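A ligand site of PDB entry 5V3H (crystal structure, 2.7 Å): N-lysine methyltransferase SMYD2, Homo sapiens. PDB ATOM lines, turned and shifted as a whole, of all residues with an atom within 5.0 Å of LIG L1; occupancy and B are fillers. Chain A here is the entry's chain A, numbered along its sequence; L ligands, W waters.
Water W3 bridges the side-chain carboxylate of Glu 146 and a nitrogen (N1) of LIG L1. Water W2 lies within hydrogen-bond range of the side-chain amide oxygen of Asn 193 (2.9 Å), an oxygen (O1) of LIG L1 (3.2 Å) and the backbone NH of Glu 146 (3.3 Å). Water W1 lies within hydrogen-bond range of O of His 218 and N4 of LIG L1.
The side-chain carboxylate (OE1) of Glu 146 sits close to an oxygen (O1) of LIG L1, at 3.2 Å. O of Ala 214 sits close to S1 of LIG L1, 3.8 Å away. A sulfur (S1) of LIG L1 sits close to the side-chain hydroxyl of Tyr 251, 3.8 Å away. Gly 27 touches LIG L1 (O to C14, 3.7 Å). OD1 of Asn 193 touches C5 of LIG L1 (3.3 Å). Leu 215 touches LIG L1 (O to C3, 3.6 Å). Met 216 touches LIG L1 (O to C4, 3.7 Å). CE2 of Phe 271 touches C13 of LIG L1, 3.1 Å away. 15 residues have an atom within 4 Å of LIG L1: Gly 27, Lys 28, Arg 30, Glu 146, His 148, Cys 192, Asn 193, Ala 214, Leu 215, Met 216, Asn 217, His 218, Tyr 251, Tyr 269 and Phe 271. The nearest printed residue that does not touch LIG L1 is Gly 29 (4.3 Å).
N1 of LIG L1 sits at hydrogen-bond distance from O of Lys 28, at 3.1 Å. N of His 218 lies within hydrogen-bond range of N3 of LIG L1, at 3.0 Å. ND2 of Asn 217 sits close to N1 of LIG L1, 3.1 Å away. A nitrogen (N1) of LIG L1 is in hydrogen-bond range of the backbone carbonyl oxygen (O) of Arg 30 (2.7 Å). The guanidinium group (NE) of Arg 30 lies within salt-bridge range of an oxygen (O2) of LIG L1, 2.9 Å away. O of Tyr 269 lies within hydrogen-bond range of O4 of LIG L1, at 2.9 Å. An oxygen (O4) of LIG L1 is in hydrogen-bond range of the side-chain sulfur (SG) of Cys 192, at 3.7 Å. A ring nitrogen (NE2) of His 148 lies within hydrogen-bond range of an oxygen (O4) of LIG L1 (2.8 Å). A nitrogen (N4) of LIG L1 sits at hydrogen-bond distance from the backbone carbonyl oxygen (O) of His 218, 3.0 Å away.
O of Glu 146 sits close to SG of Cys 192, 3.6 Å away. The side-chain amide oxygen of Asn 217 lies close to the backbone carbonyl oxygen of Arg 30. ND2 of Asn 193 lies within hydrogen-bond range of O of Glu 146 (3.2 Å). ND2 of Asn 193 lies close to SG of Cys 192 (3.6 Å). O of Met 216 is in hydrogen-bond range of OH of Tyr 251 (2.8 Å). The backbone NH (N) of Tyr 251 is in hydrogen-bond range of a ring nitrogen (ND1) of His 218 (3.1 Å).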
ATOM      1  N   GLY A  27      -1.558 -25.113   6.320  1.00  0.00           N
ATOM      2  CA  GLY A  27      -1.763 -23.729   6.734  1.00  0.00           C
ATOM      3  C   GLY A  27      -1.050 -23.306   8.002  1.00  0.00           C
ATOM      4  O   GLY A  27      -1.249 -22.183   8.446  1.00  0.00           O
ATOM      5  N   LYS A  28      -0.225 -24.177   8.600  1.00  0.00           N
ATOM      6  CA  LYS A  28       0.453 -23.879   9.865  1.00  0.00           C
ATOM      7  C   LYS A  28       1.920 -24.357   9.899  1.00  0.00           C
ATOM      8  O   LYS A  28       2.442 -24.729  10.953  1.00  0.00           O
ATOM      9  CB  LYS A  28      -0.301 -24.516  11.045  1.00  0.00           C
ATOM     10  CG  LYS A  28      -1.804 -24.309  11.051  1.00  0.00           C
ATOM     11  CD  LYS A  28      -2.395 -24.860  12.344  1.00  0.00           C
ATOM     12  CE  LYS A  28      -3.869 -24.533  12.481  1.00  0.00           C
ATOM     13  NZ  LYS A  28      -4.661 -25.218  11.425  1.00  0.00           N
ATOM     14  N   GLY A  29       2.587 -24.330   8.740  1.00  0.00           N
ATOM     15  CA  GLY A  29       3.929 -24.883   8.621  1.00  0.00           C
ATOM     16  C   GLY A  29       3.984 -26.317   9.108  1.00  0.00           C
ATOM     17  O   GLY A  29       3.134 -27.127   8.731  1.00  0.00           O
ATOM     18  N   ARG A  30       4.951 -26.618   9.973  1.00  0.00           N
ATOM     19  CA  ARG A  30       5.147 -27.957  10.540  1.00  0.00           C
ATOM     20  C   ARG A  30       4.474 -28.047  11.909  1.00  0.00           C
ATOM     21  O   ARG A  30       4.221 -27.018  12.552  1.00  0.00           O
ATOM     22  CB  ARG A  30       6.636 -28.266  10.684  1.00  0.00           C
ATOM     23  CG  ARG A  30       7.454 -28.147   9.390  1.00  0.00           C
ATOM     24  CD  ARG A  30       8.911 -27.795   9.662  1.00  0.00           C
ATOM     25  NE  ARG A  30       9.061 -26.494  10.335  1.00  0.00           N
ATOM     26  CZ  ARG A  30      10.224 -25.924  10.670  1.00  0.00           C
ATOM     27  NH1 ARG A  30      11.388 -26.520  10.393  1.00  0.00           N
ATOM     28  NH2 ARG A  30      10.230 -24.739  11.287  1.00  0.00           N
ATOM     29  N   GLY A  31       4.181 -29.270  12.329  1.00  0.00           N
ATOM     30  CA  GLY A  31       3.419 -29.514  13.562  1.00  0.00           C
ATOM     31  C   GLY A  31       3.566 -30.928  14.089  1.00  0.00           C
ATOM     32  O   GLY A  31       4.362 -31.699  13.571  1.00  0.00           O
ATOM     33  N   GLU A 146      11.769 -21.193  13.015  1.00  0.00           N
ATOM     34  CA  GLU A 146      11.213 -20.154  12.160  1.00  0.00           C
ATOM     35  C   GLU A 146      11.437 -18.747  12.722  1.00  0.00           C
ATOM     36  O   GLU A 146      11.387 -18.556  13.951  1.00  0.00           O
ATOM     37  CB  GLU A 146       9.723 -20.390  11.983  1.00  0.00           C
ATOM     38  CG  GLU A 146       9.103 -19.474  10.949  1.00  0.00           C
ATOM     39  CD  GLU A 146       7.807 -20.031  10.426  1.00  0.00           C
ATOM     40  OE1 GLU A 146       6.933 -20.389  11.253  1.00  0.00           O
ATOM     41  OE2 GLU A 146       7.673 -20.118   9.184  1.00  0.00           O
ATOM     42  N   HIS A 148      10.195 -15.462  10.957  1.00  0.00           N
ATOM     43  CA  HIS A 148       9.351 -14.381  10.436  1.00  0.00           C
ATOM     44  C   HIS A 148      10.137 -13.076  10.094  1.00  0.00           C
ATOM     45  O   HIS A 148       9.645 -11.939  10.260  1.00  0.00           O
ATOM     46  CB  HIS A 148       8.121 -14.160  11.354  1.00  0.00           C
ATOM     47  CG  HIS A 148       7.173 -15.329  11.380  1.00  0.00           C
ATOM     48  ND1 HIS A 148       6.625 -15.870  10.239  1.00  0.00           N
ATOM     49  CD2 HIS A 148       6.689 -16.058  12.411  1.00  0.00           C
ATOM     50  CE1 HIS A 148       5.842 -16.887  10.564  1.00  0.00           C
ATOM     51  NE2 HIS A 148       5.857 -17.021  11.877  1.00  0.00           N
ATOM     52  N   CYS A 192      10.113 -15.874  18.399  1.00  0.00           N
ATOM     53  CA  CYS A 192       9.064 -16.770  17.873  1.00  0.00           C
ATOM     54  C   CYS A 192       8.953 -18.090  18.652  1.00  0.00           C
ATOM     55  O   CYS A 192       7.879 -18.692  18.725  1.00  0.00           O
ATOM     56  CB  CYS A 192       9.313 -17.067  16.379  1.00  0.00           C
ATOM     57  SG  CYS A 192       8.218 -18.296  15.597  1.00  0.00           S
ATOM     58  N   ASN A 193      10.086 -18.561  19.212  1.00  0.00           N
ATOM     59  CA  ASN A 193      10.142 -19.890  19.872  1.00  0.00           C
ATOM     60  C   ASN A 193      10.465 -19.948  21.386  1.00  0.00           C
ATOM     61  O   ASN A 193      10.369 -21.026  21.996  1.00  0.00           O
ATOM     62  CB  ASN A 193      11.111 -20.770  19.100  1.00  0.00           C
ATOM     63  CG  ASN A 193      10.659 -21.023  17.666  1.00  0.00           C
ATOM     64  OD1 ASN A 193       9.959 -21.993  17.392  1.00  0.00           O
ATOM     65  ND2 ASN A 193      11.050 -20.131  16.744  1.00  0.00           N
ATOM     66  N   ALA A 214       8.471 -26.506  21.123  1.00  0.00           N
ATOM     67  CA  ALA A 214       8.121 -25.455  20.175  1.00  0.00           C
ATOM     68  C   ALA A 214       7.626 -25.956  18.821  1.00  0.00           C
ATOM     69  O   ALA A 214       7.191 -25.147  18.002  1.00  0.00           O
ATOM     70  CB  ALA A 214       9.296 -24.501  19.983  1.00  0.00           C
ATOM     71  N   LEU A 215       7.686 -27.269  18.556  1.00  0.00           N
ATOM     72  CA  LEU A 215       7.053 -27.806  17.344  1.00  0.00           C
ATOM     73  C   LEU A 215       5.524 -27.624  17.370  1.00  0.00           C
ATOM     74  O   LEU A 215       4.924 -27.395  16.318  1.00  0.00           O
ATOM     75  CB  LEU A 215       7.399 -29.285  17.116  1.00  0.00           C
ATOM     76  CG  LEU A 215       6.771 -29.967  15.881  1.00  0.00           C
ATOM     77  CD1 LEU A 215       7.144 -29.264  14.578  1.00  0.00           C
ATOM     78  CD2 LEU A 215       7.142 -31.441  15.808  1.00  0.00           C
ATOM     79  N   MET A 216       4.906 -27.728  18.555  1.00  0.00           N
ATOM     80  CA  MET A 216       3.430 -27.700  18.676  1.00  0.00           C
ATOM     81  C   MET A 216       2.872 -26.340  18.275  1.00  0.00           C
ATOM     82  O   MET A 216       3.475 -25.298  18.576  1.00  0.00           O
ATOM     83  CB  MET A 216       2.951 -28.045  20.102  1.00  0.00           C
ATOM     84  CG  MET A 216       3.301 -29.447  20.600  1.00  0.00           C
ATOM     85  SD  MET A 216       2.734 -29.820  22.269  1.00  0.00           S
ATOM     86  CE  MET A 216       3.819 -28.786  23.242  1.00  0.00           C
ATOM     87  N   ASN A 217       1.725 -26.381  17.603  1.00  0.00           N
ATOM     88  CA  ASN A 217       1.027 -25.177  17.145  1.00  0.00           C
ATOM     89  C   ASN A 217       0.018 -24.707  18.206  1.00  0.00           C
ATOM     90  O   ASN A 217      -0.133 -25.369  19.241  1.00  0.00           O
ATOM     91  CB  ASN A 217       0.345 -25.446  15.802  1.00  0.00           C
ATOM     92  CG  ASN A 217       1.339 -25.623  14.662  1.00  0.00           C
ATOM     93  OD1 ASN A 217       1.206 -26.548  13.839  1.00  0.00           O
ATOM     94  ND2 ASN A 217       2.323 -24.734  14.587  1.00  0.00           N
ATOM     95  N   HIS A 218      -0.648 -23.585  17.937  1.00  0.00           N
ATOM     96  CA  HIS A 218      -1.590 -22.936  18.868  1.00  0.00           C
ATOM     97  C   HIS A 218      -3.105 -23.171  18.651  1.00  0.00           C
ATOM     98  O   HIS A 218      -3.586 -23.154  17.523  1.00  0.00           O
ATOM     99  CB  HIS A 218      -1.392 -21.416  18.804  1.00  0.00           C
ATOM    100  CG  HIS A 218      -2.443 -20.632  19.541  1.00  0.00           C
ATOM    101  ND1 HIS A 218      -2.321 -20.337  20.875  1.00  0.00           N
ATOM    102  CD2 HIS A 218      -3.630 -20.124  19.156  1.00  0.00           C
ATOM    103  CE1 HIS A 218      -3.380 -19.650  21.279  1.00  0.00           C
ATOM    104  NE2 HIS A 218      -4.199 -19.518  20.250  1.00  0.00           N
ATOM    105  N   TYR A 251      -0.692 -20.283  23.516  1.00  0.00           N
ATOM    106  CA  TYR A 251       0.540 -19.515  23.545  1.00  0.00           C
ATOM    107  C   TYR A 251       0.309 -18.308  24.426  1.00  0.00           C
ATOM    108  O   TYR A 251       1.263 -17.586  24.701  1.00  0.00           O
ATOM    109  CB  TYR A 251       0.887 -18.987  22.139  1.00  0.00           C
ATOM    110  CG  TYR A 251       1.444 -19.953  21.100  1.00  0.00           C
ATOM    111  CD1 TYR A 251       1.495 -21.333  21.312  1.00  0.00           C
ATOM    112  CD2 TYR A 251       1.887 -19.476  19.874  1.00  0.00           C
ATOM    113  CE1 TYR A 251       2.007 -22.193  20.352  1.00  0.00           C
ATOM    114  CE2 TYR A 251       2.406 -20.325  18.900  1.00  0.00           C
ATOM    115  CZ  TYR A 251       2.463 -21.682  19.131  1.00  0.00           C
ATOM    116  OH  TYR A 251       2.966 -22.538  18.170  1.00  0.00           O
ATOM    117  N   TYR A 269       3.317 -13.334  16.927  1.00  0.00           N
ATOM    118  CA  TYR A 269       3.479 -14.596  16.143  1.00  0.00           C
ATOM    119  C   TYR A 269       3.052 -14.582  14.649  1.00  0.00           C
ATOM    120  O   TYR A 269       3.188 -15.597  13.950  1.00  0.00           O
ATOM    121  CB  TYR A 269       2.799 -15.753  16.886  1.00  0.00           C
ATOM    122  CG  TYR A 269       3.387 -16.011  18.251  1.00  0.00           C
ATOM    123  CD1 TYR A 269       4.626 -16.616  18.391  1.00  0.00           C
ATOM    124  CD2 TYR A 269       2.695 -15.656  19.419  1.00  0.00           C
ATOM    125  CE1 TYR A 269       5.176 -16.855  19.654  1.00  0.00           C
ATOM    126  CE2 TYR A 269       3.238 -15.883  20.686  1.00  0.00           C
ATOM    127  CZ  TYR A 269       4.469 -16.493  20.804  1.00  0.00           C
ATOM    128  OH  TYR A 269       5.015 -16.732  22.037  1.00  0.00           O
ATOM    129  N   PHE A 270       2.528 -13.448  14.168  1.00  0.00           N
ATOM    130  CA  PHE A 270       2.200 -13.264  12.744  1.00  0.00           C
ATOM    131  C   PHE A 270       1.206 -14.285  12.158  1.00  0.00           C
ATOM    132  O   PHE A 270       1.423 -14.837  11.098  1.00  0.00           O
ATOM    133  CB  PHE A 270       3.503 -13.207  11.936  1.00  0.00           C
ATOM    134  CG  PHE A 270       4.489 -12.172  12.433  1.00  0.00           C
ATOM    135  CD1 PHE A 270       4.434 -10.869  11.971  1.00  0.00           C
ATOM    136  CD2 PHE A 270       5.450 -12.504  13.366  1.00  0.00           C
ATOM    137  CE1 PHE A 270       5.326  -9.909  12.428  1.00  0.00           C
ATOM    138  CE2 PHE A 270       6.349 -11.546  13.838  1.00  0.00           C
ATOM    139  CZ  PHE A 270       6.282 -10.247  13.368  1.00  0.00           C
ATOM    140  N   PHE A 271       0.123 -14.556  12.892  1.00  0.00           N
ATOM    141  CA  PHE A 271      -0.945 -15.420  12.366  1.00  0.00           C
ATOM    142  C   PHE A 271      -2.308 -15.130  13.002  1.00  0.00           C
ATOM    143  O   PHE A 271      -2.405 -14.495  14.055  1.00  0.00           O
ATOM    144  CB  PHE A 271      -0.578 -16.920  12.462  1.00  0.00           C
ATOM    145  CG  PHE A 271      -0.890 -17.548  13.801  1.00  0.00           C
ATOM    146  CD1 PHE A 271       0.039 -17.544  14.827  1.00  0.00           C
ATOM    147  CD2 PHE A 271      -2.116 -18.168  14.019  1.00  0.00           C
ATOM    148  CE1 PHE A 271      -0.240 -18.132  16.050  1.00  0.00           C
ATOM    149  CE2 PHE A 271      -2.422 -18.744  15.236  1.00  0.00           C
ATOM    150  CZ  PHE A 271      -1.474 -18.726  16.256  1.00  0.00           C
ATOM    151  N   THR A 272      -3.358 -15.596  12.317  1.00  0.00           N
ATOM    152  CA  THR A 272      -4.741 -15.466  12.755  1.00  0.00           C
ATOM    153  C   THR A 272      -5.278 -16.868  13.084  1.00  0.00           C
ATOM    154  O   THR A 272      -5.288 -17.746  12.214  1.00  0.00           O
ATOM    155  CB  THR A 272      -5.612 -14.834  11.642  1.00  0.00           C
ATOM    156  OG1 THR A 272      -4.988 -13.625  11.166  1.00  0.00           O
ATOM    157  CG2 THR A 272      -7.023 -14.514  12.151  1.00  0.00           C
ATOM    158  N   CYS A 273      -5.731 -17.048  14.332  1.00  0.00           N
ATOM    159  CA  CYS A 273      -6.303 -18.323  14.790  1.00  0.00           C
ATOM    160  C   CYS A 273      -7.724 -18.553  14.247  1.00  0.00           C
ATOM    161  O   CYS A 273      -8.556 -17.646  14.286  1.00  0.00           O
ATOM    162  CB  CYS A 273      -6.313 -18.360  16.323  1.00  0.00           C
ATOM    163  SG  CYS A 273      -6.926 -19.907  17.007  1.00  0.00           S
HETATM  164  N1  LIG L   1       4.867 -24.461  12.875  1.00  0.00           N
HETATM  165  C1  LIG L   1       6.014 -23.857  13.512  1.00  0.00           C
HETATM  166  C2  LIG L   1       7.243 -24.195  12.712  1.00  0.00           C
HETATM  167  O1  LIG L   1       7.944 -23.256  12.284  1.00  0.00           O
HETATM  168  O2  LIG L   1       7.521 -25.396  12.515  1.00  0.00           O
HETATM  169  C3  LIG L   1       6.180 -24.330  14.959  1.00  0.00           C
HETATM  170  C4  LIG L   1       5.388 -23.460  15.933  1.00  0.00           C
HETATM  171  S1  LIG L   1       6.151 -22.017  16.210  1.00  0.00           S
HETATM  172  C5  LIG L   1       6.662 -21.980  17.789  1.00  0.00           C
HETATM  173  C6  LIG L   1       5.115 -20.728  15.992  1.00  0.00           C
HETATM  174  C7  LIG L   1       4.673 -20.483  14.550  1.00  0.00           C
HETATM  175  O3  LIG L   1       3.798 -21.501  14.046  1.00  0.00           O
HETATM  176  C8  LIG L   1       3.893 -19.202  14.429  1.00  0.00           C
HETATM  177  O4  LIG L   1       4.748 -18.080  14.208  1.00  0.00           O
HETATM  178  C9  LIG L   1       2.951 -19.459  13.277  1.00  0.00           C
HETATM  179  O5  LIG L   1       3.564 -19.137  12.018  1.00  0.00           O
HETATM  180  C10 LIG L   1       2.704 -20.950  13.322  1.00  0.00           C
HETATM  181  N2  LIG L   1       1.395 -21.291  13.959  1.00  0.00           N
HETATM  182  C11 LIG L   1       1.209 -21.798  15.184  1.00  0.00           C
HETATM  183  N3  LIG L   1      -0.109 -21.994  15.446  1.00  0.00           N
HETATM  184  C12 LIG L   1      -0.791 -21.617  14.361  1.00  0.00           C
HETATM  185  C13 LIG L   1      -2.218 -21.584  13.954  1.00  0.00           C
HETATM  186  N4  LIG L   1      -3.196 -21.985  14.801  1.00  0.00           N
HETATM  187  N5  LIG L   1      -2.519 -21.111  12.718  1.00  0.00           N
HETATM  188  C14 LIG L   1      -1.555 -20.696  11.861  1.00  0.00           C
HETATM  189  N6  LIG L   1      -0.234 -20.716  12.163  1.00  0.00           N
HETATM  190  C15 LIG L   1       0.198 -21.160  13.372  1.00  0.00           C
HETATM  191  C1  LG2 L   2       0.699 -23.574  39.455  1.00  0.00           C
HETATM  192  C2  LG2 L   2       1.988 -24.105  39.527  1.00  0.00           C
HETATM  193  C3  LG2 L   2       2.998 -23.624  38.703  1.00  0.00           C
HETATM  194  C4  LG2 L   2       2.733 -22.620  37.782  1.00  0.00           C
HETATM  195  C5  LG2 L   2       3.857 -22.110  36.906  1.00  0.00           C
HETATM  196  C6  LG2 L   2       3.286 -21.042  34.718  1.00  0.00           C
HETATM  197 CL1  LG2 L   2      -0.553 -24.184  40.498  1.00  0.00          CL
HETATM  198  N1  LG2 L   2       3.628 -22.110  35.457  1.00  0.00           N
HETATM  199  C7  LG2 L   2       3.211 -21.412  33.422  1.00  0.00           C
HETATM  200  C8  LG2 L   2       2.841 -20.489  32.287  1.00  0.00           C
HETATM  201  N2  LG2 L   2       4.020 -20.022  31.534  1.00  0.00           N
HETATM  202  C9  LG2 L   2       3.652 -19.139  30.412  1.00  0.00           C
HETATM  203  C10 LG2 L   2       4.821 -19.738  29.631  1.00  0.00           C
HETATM  204  C11 LG2 L   2       4.562 -20.954  30.539  1.00  0.00           C
HETATM  205  N3  LG2 L   2       4.563 -20.028  28.210  1.00  0.00           N
HETATM  206  C12 LG2 L   2       5.315 -19.537  27.195  1.00  0.00           C
HETATM  207  O1  LG2 L   2       6.270 -18.797  27.403  1.00  0.00           O
HETATM  208  C13 LG2 L   2       5.022 -19.911  25.802  1.00  0.00           C
HETATM  209  C14 LG2 L   2       5.932 -19.841  24.811  1.00  0.00           C
HETATM  210  N4  LG2 L   2       5.343 -20.266  23.691  1.00  0.00           N
HETATM  211  N5  LG2 L   2       4.030 -20.610  24.025  1.00  0.00           N
HETATM  212  N6  LG2 L   2       3.865 -20.386  25.283  1.00  0.00           N
HETATM  213  C15 LG2 L   2       6.029 -20.351  22.406  1.00  0.00           C
HETATM  214  C16 LG2 L   2       5.467 -21.379  21.417  1.00  0.00           C
HETATM  215  C17 LG2 L   2       5.279 -19.881  21.161  1.00  0.00           C
HETATM  216  C18 LG2 L   2       3.523 -22.784  33.377  1.00  0.00           C
HETATM  217  N7  LG2 L   2       3.768 -23.194  34.588  1.00  0.00           N
HETATM  218  C19 LG2 L   2       1.459 -22.080  37.711  1.00  0.00           C
HETATM  219  C20 LG2 L   2       0.449 -22.562  38.535  1.00  0.00           C
HETATM  220  O   HOH W   1      -5.960 -23.660  16.052  1.00  0.00           O
HETATM  221  O   HOH W   2       9.946 -23.270  14.823  1.00  0.00           O
HETATM  222  O   HOH W   3       4.922 -22.163  11.138  1.00  0.00           O
